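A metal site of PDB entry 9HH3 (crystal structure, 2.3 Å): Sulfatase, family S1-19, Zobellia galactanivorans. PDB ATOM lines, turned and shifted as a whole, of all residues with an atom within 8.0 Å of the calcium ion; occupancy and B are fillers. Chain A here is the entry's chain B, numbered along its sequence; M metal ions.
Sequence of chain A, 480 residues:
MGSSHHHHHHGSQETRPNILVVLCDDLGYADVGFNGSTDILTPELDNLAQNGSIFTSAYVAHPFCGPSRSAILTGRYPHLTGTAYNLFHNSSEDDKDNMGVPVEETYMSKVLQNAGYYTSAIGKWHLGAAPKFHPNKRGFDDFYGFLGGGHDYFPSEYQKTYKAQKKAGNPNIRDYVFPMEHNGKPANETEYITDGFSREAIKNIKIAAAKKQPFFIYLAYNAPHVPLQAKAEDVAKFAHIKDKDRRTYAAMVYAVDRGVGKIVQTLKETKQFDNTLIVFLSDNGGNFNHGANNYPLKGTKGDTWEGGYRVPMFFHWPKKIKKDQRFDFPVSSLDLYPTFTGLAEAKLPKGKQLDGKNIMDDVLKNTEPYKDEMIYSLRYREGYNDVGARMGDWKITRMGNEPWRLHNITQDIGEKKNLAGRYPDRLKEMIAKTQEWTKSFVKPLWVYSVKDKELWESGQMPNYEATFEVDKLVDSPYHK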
ATOM      1  N   LEU A  23       5.738  -8.804 -18.381  1.00  0.00           N
ATOM      2  CA  LEU A  23       5.694  -9.313 -17.006  1.00  0.00           C
ATOM      3  C   LEU A  23       6.187 -10.761 -16.987  1.00  0.00           C
ATOM      4  O   LEU A  23       5.495 -11.653 -17.516  1.00  0.00           O
ATOM      5  CB  LEU A  23       4.264  -9.224 -16.472  1.00  0.00           C
ATOM      6  CG  LEU A  23       4.068  -9.702 -15.036  1.00  0.00           C
ATOM      7  CD1 LEU A  23       4.885  -8.798 -14.090  1.00  0.00           C
ATOM      8  CD2 LEU A  23       2.580  -9.750 -14.653  1.00  0.00           C
ATOM      9  N   CYS A  24       7.330 -11.009 -16.368  1.00  0.00           N
ATOM     10  CA  CYS A  24       7.805 -12.374 -16.189  1.00  0.00           C
ATOM     11  C   CYS A  24       7.259 -12.983 -14.895  1.00  0.00           C
ATOM     12  O   CYS A  24       6.793 -12.275 -14.005  1.00  0.00           O
ATOM     13  CB  CYS A  24       9.325 -12.442 -16.177  1.00  0.00           C
ATOM     14  SG  CYS A  24      10.043 -12.281 -17.779  1.00  0.00           S
ATOM     15  N   ASP A  25       7.406 -14.312 -14.760  1.00  0.00           N
ATOM     16  CA  ASP A  25       6.780 -15.056 -13.666  1.00  0.00           C
ATOM     17  C   ASP A  25       7.861 -15.727 -12.812  1.00  0.00           C
ATOM     18  O   ASP A  25       8.457 -16.724 -13.233  1.00  0.00           O
ATOM     19  CB  ASP A  25       5.810 -16.097 -14.239  1.00  0.00           C
ATOM     20  CG  ASP A  25       4.863 -16.663 -13.178  1.00  0.00           C
ATOM     21  OD1 ASP A  25       5.012 -16.286 -12.003  1.00  0.00           O
ATOM     22  OD2 ASP A  25       3.937 -17.449 -13.524  1.00  0.00           O
ATOM     23  N   ASP A  26       8.057 -15.220 -11.587  1.00  0.00           N
ATOM     24  CA  ASP A  26       9.059 -15.735 -10.636  1.00  0.00           C
ATOM     25  C   ASP A  26      10.506 -15.459 -11.076  1.00  0.00           C
ATOM     26  O   ASP A  26      11.410 -16.213 -10.736  1.00  0.00           O
ATOM     27  CB  ASP A  26       8.894 -17.240 -10.384  1.00  0.00           C
ATOM     28  CG  ASP A  26       7.587 -17.593  -9.707  1.00  0.00           C
ATOM     29  OD1 ASP A  26       6.754 -16.695  -9.456  1.00  0.00           O
ATOM     30  OD2 ASP A  26       7.395 -18.776  -9.392  1.00  0.00           O
ATOM     31  N   LEU A  27      10.747 -14.372 -11.795  1.00  0.00           N
ATOM     32  CA  LEU A  27      12.119 -14.019 -12.157  1.00  0.00           C
ATOM     33  C   LEU A  27      12.857 -13.469 -10.940  1.00  0.00           C
ATOM     34  O   LEU A  27      12.368 -12.549 -10.263  1.00  0.00           O
ATOM     35  CB  LEU A  27      12.097 -12.999 -13.273  1.00  0.00           C
ATOM     36  CG  LEU A  27      13.440 -12.440 -13.741  1.00  0.00           C
ATOM     37  CD1 LEU A  27      14.094 -13.453 -14.643  1.00  0.00           C
ATOM     38  CD2 LEU A  27      13.201 -11.084 -14.457  1.00  0.00           C
ATOM     39  N   HIS A  62       2.472  -7.930  -3.518  1.00  0.00           N
ATOM     40  CA  HIS A  62       2.347  -9.165  -2.759  1.00  0.00           C
ATOM     41  C   HIS A  62       3.446 -10.103  -3.215  1.00  0.00           C
ATOM     42  O   HIS A  62       3.825 -10.068  -4.403  1.00  0.00           O
ATOM     43  CB  HIS A  62       0.951  -9.790  -2.937  1.00  0.00           C
ATOM     44  CG  HIS A  62       0.580 -10.781  -1.874  1.00  0.00           C
ATOM     45  ND1 HIS A  62       0.214 -10.400  -0.594  1.00  0.00           N
ATOM     46  CD2 HIS A  62       0.469 -12.133  -1.906  1.00  0.00           C
ATOM     47  CE1 HIS A  62      -0.070 -11.473   0.118  1.00  0.00           C
ATOM     48  NE2 HIS A  62       0.062 -12.538  -0.652  1.00  0.00           N
ATOM     49  N   PRO A  63       4.025 -10.914  -2.325  1.00  0.00           N
ATOM     50  CA  PRO A  63       5.168 -11.738  -2.737  1.00  0.00           C
ATOM     51  C   PRO A  63       4.820 -13.032  -3.470  1.00  0.00           C
ATOM     52  O   PRO A  63       5.685 -13.903  -3.491  1.00  0.00           O
ATOM     53  CB  PRO A  63       5.876 -12.043  -1.401  1.00  0.00           C
ATOM     54  CG  PRO A  63       4.767 -12.012  -0.361  1.00  0.00           C
ATOM     55  CD  PRO A  63       3.838 -10.892  -0.862  1.00  0.00           C
ATOM     56  N   PHE A  64       3.606 -13.223  -4.036  1.00  0.00           N
ATOM     57  CA  PHE A  64       3.428 -14.356  -4.952  1.00  0.00           C
ATOM     58  C   PHE A  64       2.272 -14.080  -5.934  1.00  0.00           C
ATOM     59  O   PHE A  64       1.569 -13.079  -5.821  1.00  0.00           O
ATOM     60  CB  PHE A  64       3.264 -15.697  -4.208  1.00  0.00           C
ATOM     61  CG  PHE A  64       2.093 -15.761  -3.277  1.00  0.00           C
ATOM     62  CD1 PHE A  64       0.815 -16.014  -3.762  1.00  0.00           C
ATOM     63  CD2 PHE A  64       2.258 -15.578  -1.903  1.00  0.00           C
ATOM     64  CE1 PHE A  64      -0.290 -16.084  -2.916  1.00  0.00           C
ATOM     65  CE2 PHE A  64       1.156 -15.642  -1.039  1.00  0.00           C
ATOM     66  CZ  PHE A  64      -0.127 -15.890  -1.555  1.00  0.00           C
ATOM     67  N   DDZ A  65       2.092 -15.040  -6.866  1.00  0.00           N
ATOM     68  CA  DDZ A  65       1.448 -14.936  -8.200  1.00  0.00           C
ATOM     69  C   DDZ A  65       0.117 -14.161  -8.161  1.00  0.00           C
ATOM     70  O   DDZ A  65       0.122 -12.959  -8.488  1.00  0.00           O
ATOM     71  OG1 DDZ A  65       0.294 -16.269  -9.892  1.00  0.00           O
ATOM     72  OG2 DDZ A  65       2.407 -16.992  -9.161  1.00  0.00           O
ATOM     73  CB  DDZ A  65       1.198 -16.341  -8.794  1.00  0.00           C
ATOM     74  N   GLY A  66      -0.963 -14.847  -7.822  1.00  0.00           N
ATOM     75  CA  GLY A  66      -2.312 -14.323  -7.941  1.00  0.00           C
ATOM     76  C   GLY A  66      -2.559 -12.927  -7.391  1.00  0.00           C
ATOM     77  O   GLY A  66      -3.057 -12.047  -8.084  1.00  0.00           O
ATOM     78  N   SER A  68      -0.386 -10.588  -6.581  1.00  0.00           N
ATOM     79  CA  SER A  68       0.415  -9.585  -7.263  1.00  0.00           C
ATOM     80  C   SER A  68      -0.246  -9.181  -8.583  1.00  0.00           C
ATOM     81  O   SER A  68      -0.369  -7.986  -8.896  1.00  0.00           O
ATOM     82  CB  SER A  68       1.859 -10.070  -7.457  1.00  0.00           C
ATOM     83  OG  SER A  68       2.620  -9.168  -8.241  1.00  0.00           O
ATOM     84  N   ARG A  69      -0.737 -10.160  -9.337  1.00  0.00           N
ATOM     85  CA  ARG A  69      -1.396  -9.857 -10.597  1.00  0.00           C
ATOM     86  C   ARG A  69      -2.730  -9.146 -10.371  1.00  0.00           C
ATOM     87  O   ARG A  69      -3.056  -8.178 -11.067  1.00  0.00           O
ATOM     88  CB  ARG A  69      -1.561 -11.141 -11.399  1.00  0.00           C
ATOM     89  CG  ARG A  69      -0.207 -11.621 -11.894  1.00  0.00           C
ATOM     90  CD  ARG A  69      -0.180 -13.109 -12.199  1.00  0.00           C
ATOM     91  NE  ARG A  69       1.205 -13.547 -12.342  1.00  0.00           N
ATOM     92  CZ  ARG A  69       1.898 -13.492 -13.467  1.00  0.00           C
ATOM     93  NH1 ARG A  69       1.333 -13.144 -14.610  1.00  0.00           N
ATOM     94  NH2 ARG A  69       3.190 -13.807 -13.448  1.00  0.00           N
ATOM     95  N   ASN A  86      -3.969 -17.175  -3.502  1.00  0.00           N
ATOM     96  CA  ASN A  86      -4.051 -17.712  -4.845  1.00  0.00           C
ATOM     97  C   ASN A  86      -5.320 -18.534  -5.024  1.00  0.00           C
ATOM     98  O   ASN A  86      -5.758 -19.251  -4.119  1.00  0.00           O
ATOM     99  CB  ASN A  86      -2.846 -18.605  -5.155  1.00  0.00           C
ATOM    100  CG  ASN A  86      -1.687 -17.836  -5.763  1.00  0.00           C
ATOM    101  OD1 ASN A  86      -1.849 -16.704  -6.199  1.00  0.00           O
ATOM    102  ND2 ASN A  86      -0.511 -18.437  -5.780  1.00  0.00           N
ATOM    103  N   LYS A 124      -0.216 -15.828 -19.309  1.00  0.00           N
ATOM    104  CA  LYS A 124      -0.826 -16.254 -18.054  1.00  0.00           C
ATOM    105  C   LYS A 124      -1.867 -15.258 -17.540  1.00  0.00           C
ATOM    106  O   LYS A 124      -1.635 -14.047 -17.574  1.00  0.00           O
ATOM    107  CB  LYS A 124       0.270 -16.442 -17.001  1.00  0.00           C
ATOM    108  CG  LYS A 124      -0.194 -16.537 -15.549  1.00  0.00           C
ATOM    109  CD  LYS A 124       1.003 -16.877 -14.630  1.00  0.00           C
ATOM    110  CE  LYS A 124       0.627 -16.943 -13.140  1.00  0.00           C
ATOM    111  NZ  LYS A 124       1.751 -17.520 -12.289  1.00  0.00           N
ATOM    112  N   HIS A 126      -4.707 -16.146 -14.414  1.00  0.00           N
ATOM    113  CA  HIS A 126      -4.787 -16.479 -12.998  1.00  0.00           C
ATOM    114  C   HIS A 126      -5.657 -15.500 -12.215  1.00  0.00           C
ATOM    115  O   HIS A 126      -5.485 -15.356 -11.000  1.00  0.00           O
ATOM    116  CB  HIS A 126      -3.405 -16.573 -12.351  1.00  0.00           C
ATOM    117  CG  HIS A 126      -3.356 -17.464 -11.140  1.00  0.00           C
ATOM    118  ND1 HIS A 126      -2.323 -17.440 -10.230  1.00  0.00           N
ATOM    119  CD2 HIS A 126      -4.205 -18.448 -10.728  1.00  0.00           C
ATOM    120  CE1 HIS A 126      -2.561 -18.336  -9.280  1.00  0.00           C
ATOM    121  NE2 HIS A 126      -3.693 -18.963  -9.560  1.00  0.00           N
ATOM    122  N   GLY A 149      -2.748 -20.800 -13.397  1.00  0.00           N
ATOM    123  CA  GLY A 149      -1.536 -20.268 -12.799  1.00  0.00           C
ATOM    124  C   GLY A 149      -0.233 -20.729 -13.438  1.00  0.00           C
ATOM    125  O   GLY A 149       0.833 -20.185 -13.123  1.00  0.00           O
ATOM    126  N   TYR A 221       4.309 -13.522 -19.716  1.00  0.00           N
ATOM    127  CA  TYR A 221       5.049 -14.774 -19.828  1.00  0.00           C
ATOM    128  C   TYR A 221       4.907 -15.630 -18.570  1.00  0.00           C
ATOM    129  O   TYR A 221       5.043 -15.135 -17.447  1.00  0.00           O
ATOM    130  CB  TYR A 221       6.537 -14.518 -20.048  1.00  0.00           C
ATOM    131  CG  TYR A 221       6.921 -13.941 -21.399  1.00  0.00           C
ATOM    132  CD1 TYR A 221       6.893 -14.733 -22.543  1.00  0.00           C
ATOM    133  CD2 TYR A 221       7.378 -12.629 -21.514  1.00  0.00           C
ATOM    134  CE1 TYR A 221       7.300 -14.240 -23.748  1.00  0.00           C
ATOM    135  CE2 TYR A 221       7.771 -12.111 -22.734  1.00  0.00           C
ATOM    136  CZ  TYR A 221       7.730 -12.926 -23.859  1.00  0.00           C
ATOM    137  OH  TYR A 221       8.134 -12.439 -25.082  1.00  0.00           O
ATOM    138  N   ASN A 222       4.723 -16.943 -18.759  1.00  0.00           N
ATOM    139  CA  ASN A 222       4.819 -17.796 -17.588  1.00  0.00           C
ATOM    140  C   ASN A 222       6.272 -18.160 -17.258  1.00  0.00           C
ATOM    141  O   ASN A 222       6.559 -18.545 -16.127  1.00  0.00           O
ATOM    142  CB  ASN A 222       3.955 -19.061 -17.749  1.00  0.00           C
ATOM    143  CG  ASN A 222       4.419 -19.962 -18.900  1.00  0.00           C
ATOM    144  OD1 ASN A 222       4.780 -19.498 -19.983  1.00  0.00           O
ATOM    145  ND2 ASN A 222       4.405 -21.278 -18.666  1.00  0.00           N
ATOM    146  N   HIS A 225       8.745 -19.538 -14.533  1.00  0.00           N
ATOM    147  CA  HIS A 225       8.006 -20.345 -13.569  1.00  0.00           C
ATOM    148  C   HIS A 225       8.109 -21.835 -13.898  1.00  0.00           C
ATOM    149  O   HIS A 225       8.218 -22.221 -15.075  1.00  0.00           O
ATOM    150  CB  HIS A 225       6.537 -19.877 -13.566  1.00  0.00           C
ATOM    151  CG  HIS A 225       5.673 -20.445 -12.477  1.00  0.00           C
ATOM    152  ND1 HIS A 225       5.272 -21.770 -12.453  1.00  0.00           N
ATOM    153  CD2 HIS A 225       5.044 -19.842 -11.433  1.00  0.00           C
ATOM    154  CE1 HIS A 225       4.474 -21.959 -11.420  1.00  0.00           C
ATOM    155  NE2 HIS A 225       4.320 -20.807 -10.786  1.00  0.00           N
ATOM    156  N   SER A 282       9.160  -8.289 -12.891  1.00  0.00           N
ATOM    157  CA  SER A 282       8.731  -9.590 -12.426  1.00  0.00           C
ATOM    158  C   SER A 282       7.516  -9.478 -11.505  1.00  0.00           C
ATOM    159  O   SER A 282       7.304  -8.446 -10.859  1.00  0.00           O
ATOM    160  CB  SER A 282       9.849 -10.292 -11.676  1.00  0.00           C
ATOM    161  OG  SER A 282       9.362 -11.546 -11.287  1.00  0.00           O
ATOM    162  N   ASP A 283       6.697 -10.529 -11.449  1.00  0.00           N
ATOM    163  CA  ASP A 283       5.493 -10.419 -10.636  1.00  0.00           C
ATOM    164  C   ASP A 283       5.746 -10.673  -9.155  1.00  0.00           C
ATOM    165  O   ASP A 283       4.884 -10.361  -8.335  1.00  0.00           O
ATOM    166  CB  ASP A 283       4.387 -11.345 -11.132  1.00  0.00           C
ATOM    167  CG  ASP A 283       4.682 -12.823 -10.856  1.00  0.00           C
ATOM    168  OD1 ASP A 283       5.870 -13.241 -10.800  1.00  0.00           O
ATOM    169  OD2 ASP A 283       3.706 -13.585 -10.715  1.00  0.00           O
ATOM    170  N   ASN A 284       6.890 -11.262  -8.801  1.00  0.00           N
ATOM    171  CA  ASN A 284       7.269 -11.466  -7.411  1.00  0.00           C
ATOM    172  C   ASN A 284       8.730 -11.904  -7.441  1.00  0.00           C
ATOM    173  O   ASN A 284       9.317 -12.020  -8.509  1.00  0.00           O
ATOM    174  CB  ASN A 284       6.340 -12.478  -6.723  1.00  0.00           C
ATOM    175  CG  ASN A 284       6.276 -13.798  -7.459  1.00  0.00           C
ATOM    176  OD1 ASN A 284       7.274 -14.545  -7.571  1.00  0.00           O
ATOM    177  ND2 ASN A 284       5.080 -14.138  -7.924  1.00  0.00           N
ATOM    178  N   GLY A 285       9.330 -12.080  -6.258  1.00  0.00           N
ATOM    179  CA  GLY A 285      10.721 -12.491  -6.199  1.00  0.00           C
ATOM    180  C   GLY A 285      10.925 -13.907  -6.694  1.00  0.00           C
ATOM    181  O   GLY A 285       9.992 -14.708  -6.761  1.00  0.00           O
ATOM    182  N   GLY A 286      12.162 -14.233  -7.053  1.00  0.00           N
ATOM    183  CA  GLY A 286      12.463 -15.572  -7.524  1.00  0.00           C
ATOM    184  C   GLY A 286      12.328 -16.616  -6.436  1.00  0.00           C
ATOM    185  O   GLY A 286      12.583 -16.360  -5.257  1.00  0.00           O
ATOM    186  N   ASN A 287      11.919 -17.820  -6.835  1.00  0.00           N
ATOM    187  CA  ASN A 287      11.892 -18.980  -5.956  1.00  0.00           C
ATOM    188  C   ASN A 287      13.276 -19.612  -6.003  1.00  0.00           C
ATOM    189  O   ASN A 287      13.645 -20.192  -7.026  1.00  0.00           O
ATOM    190  CB  ASN A 287      10.828 -19.981  -6.376  1.00  0.00           C
ATOM    191  CG  ASN A 287      10.688 -21.150  -5.389  1.00  0.00           C
ATOM    192  OD1 ASN A 287      11.659 -21.562  -4.725  1.00  0.00           O
ATOM    193  ND2 ASN A 287       9.485 -21.722  -5.333  1.00  0.00           N
ATOM    194  N   LYS A 301      10.693 -16.209  -3.105  1.00  0.00           N
ATOM    195  CA  LYS A 301       9.281 -16.025  -3.444  1.00  0.00           C
ATOM    196  C   LYS A 301       8.411 -16.357  -2.251  1.00  0.00           C
ATOM    197  O   LYS A 301       8.585 -17.402  -1.611  1.00  0.00           O
ATOM    198  CB  LYS A 301       8.917 -16.922  -4.613  1.00  0.00           C
ATOM    199  CG  LYS A 301       7.417 -17.076  -4.831  1.00  0.00           C
ATOM    200  CD  LYS A 301       7.193 -17.984  -6.022  1.00  0.00           C
ATOM    201  CE  LYS A 301       5.719 -18.255  -6.285  1.00  0.00           C
ATOM    202  NZ  LYS A 301       5.481 -19.059  -7.525  1.00  0.00           N
HETATM  203 CA    CA M   1       4.919 -15.389  -9.790  1.00  0.00          CA
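The side-chain carboxylate of Asp 25 is in salt-bridge range of the guanidinium group of Arg 69 (3.7 Å). OG1 of DDZ 65 is in hydrogen-bond range of the side-chain amino group (NZ) of Lys 124. The backbone NH (N) of Asp 283 sits at hydrogen-bond distance from the backbone carbonyl oxygen (O) of Cys 24 (3.1 Å). O of Asn 284 is in hydrogen-bond range of OG of Ser 282 (2.8 Å). The side-chain carboxylate (OD2) of Asp 25 lies within salt-bridge range of the side-chain amino group (NZ) of Lys 124 (2.5 Å). OD2 of Asp 26 is in salt-bridge range of NZ of Lys 301, at 2.7 Å. The side-chain amide nitrogen of Asn 284 sits close to N of DDZ 65 (3.3 Å). The guanidinium group of Arg 69 sits close to the side-chain carboxylate of Asp 283 (2.8 Å).
Within 4 Å of the calcium ion: Asp 25, Asp 26, DDZ 65, Asp 283 and Asn 284. The nearest printed residue that does not touch the calcium ion is Arg 69 (4.3 Å).
The calcium ion is bound by the side-chain amide nitrogen (ND2) of Asn 284, the side-chain carboxylate (OD1) of Asp 26, the side-chain carboxylate (OD2) of Asp 283, the side-chain carboxylate (OD1) of Asp 25 and the side-chain carboxylate (OD1) of Asp 283. Slightly farther from the calcium ion lies OG2 of DDZ 65 (3.0 Å).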
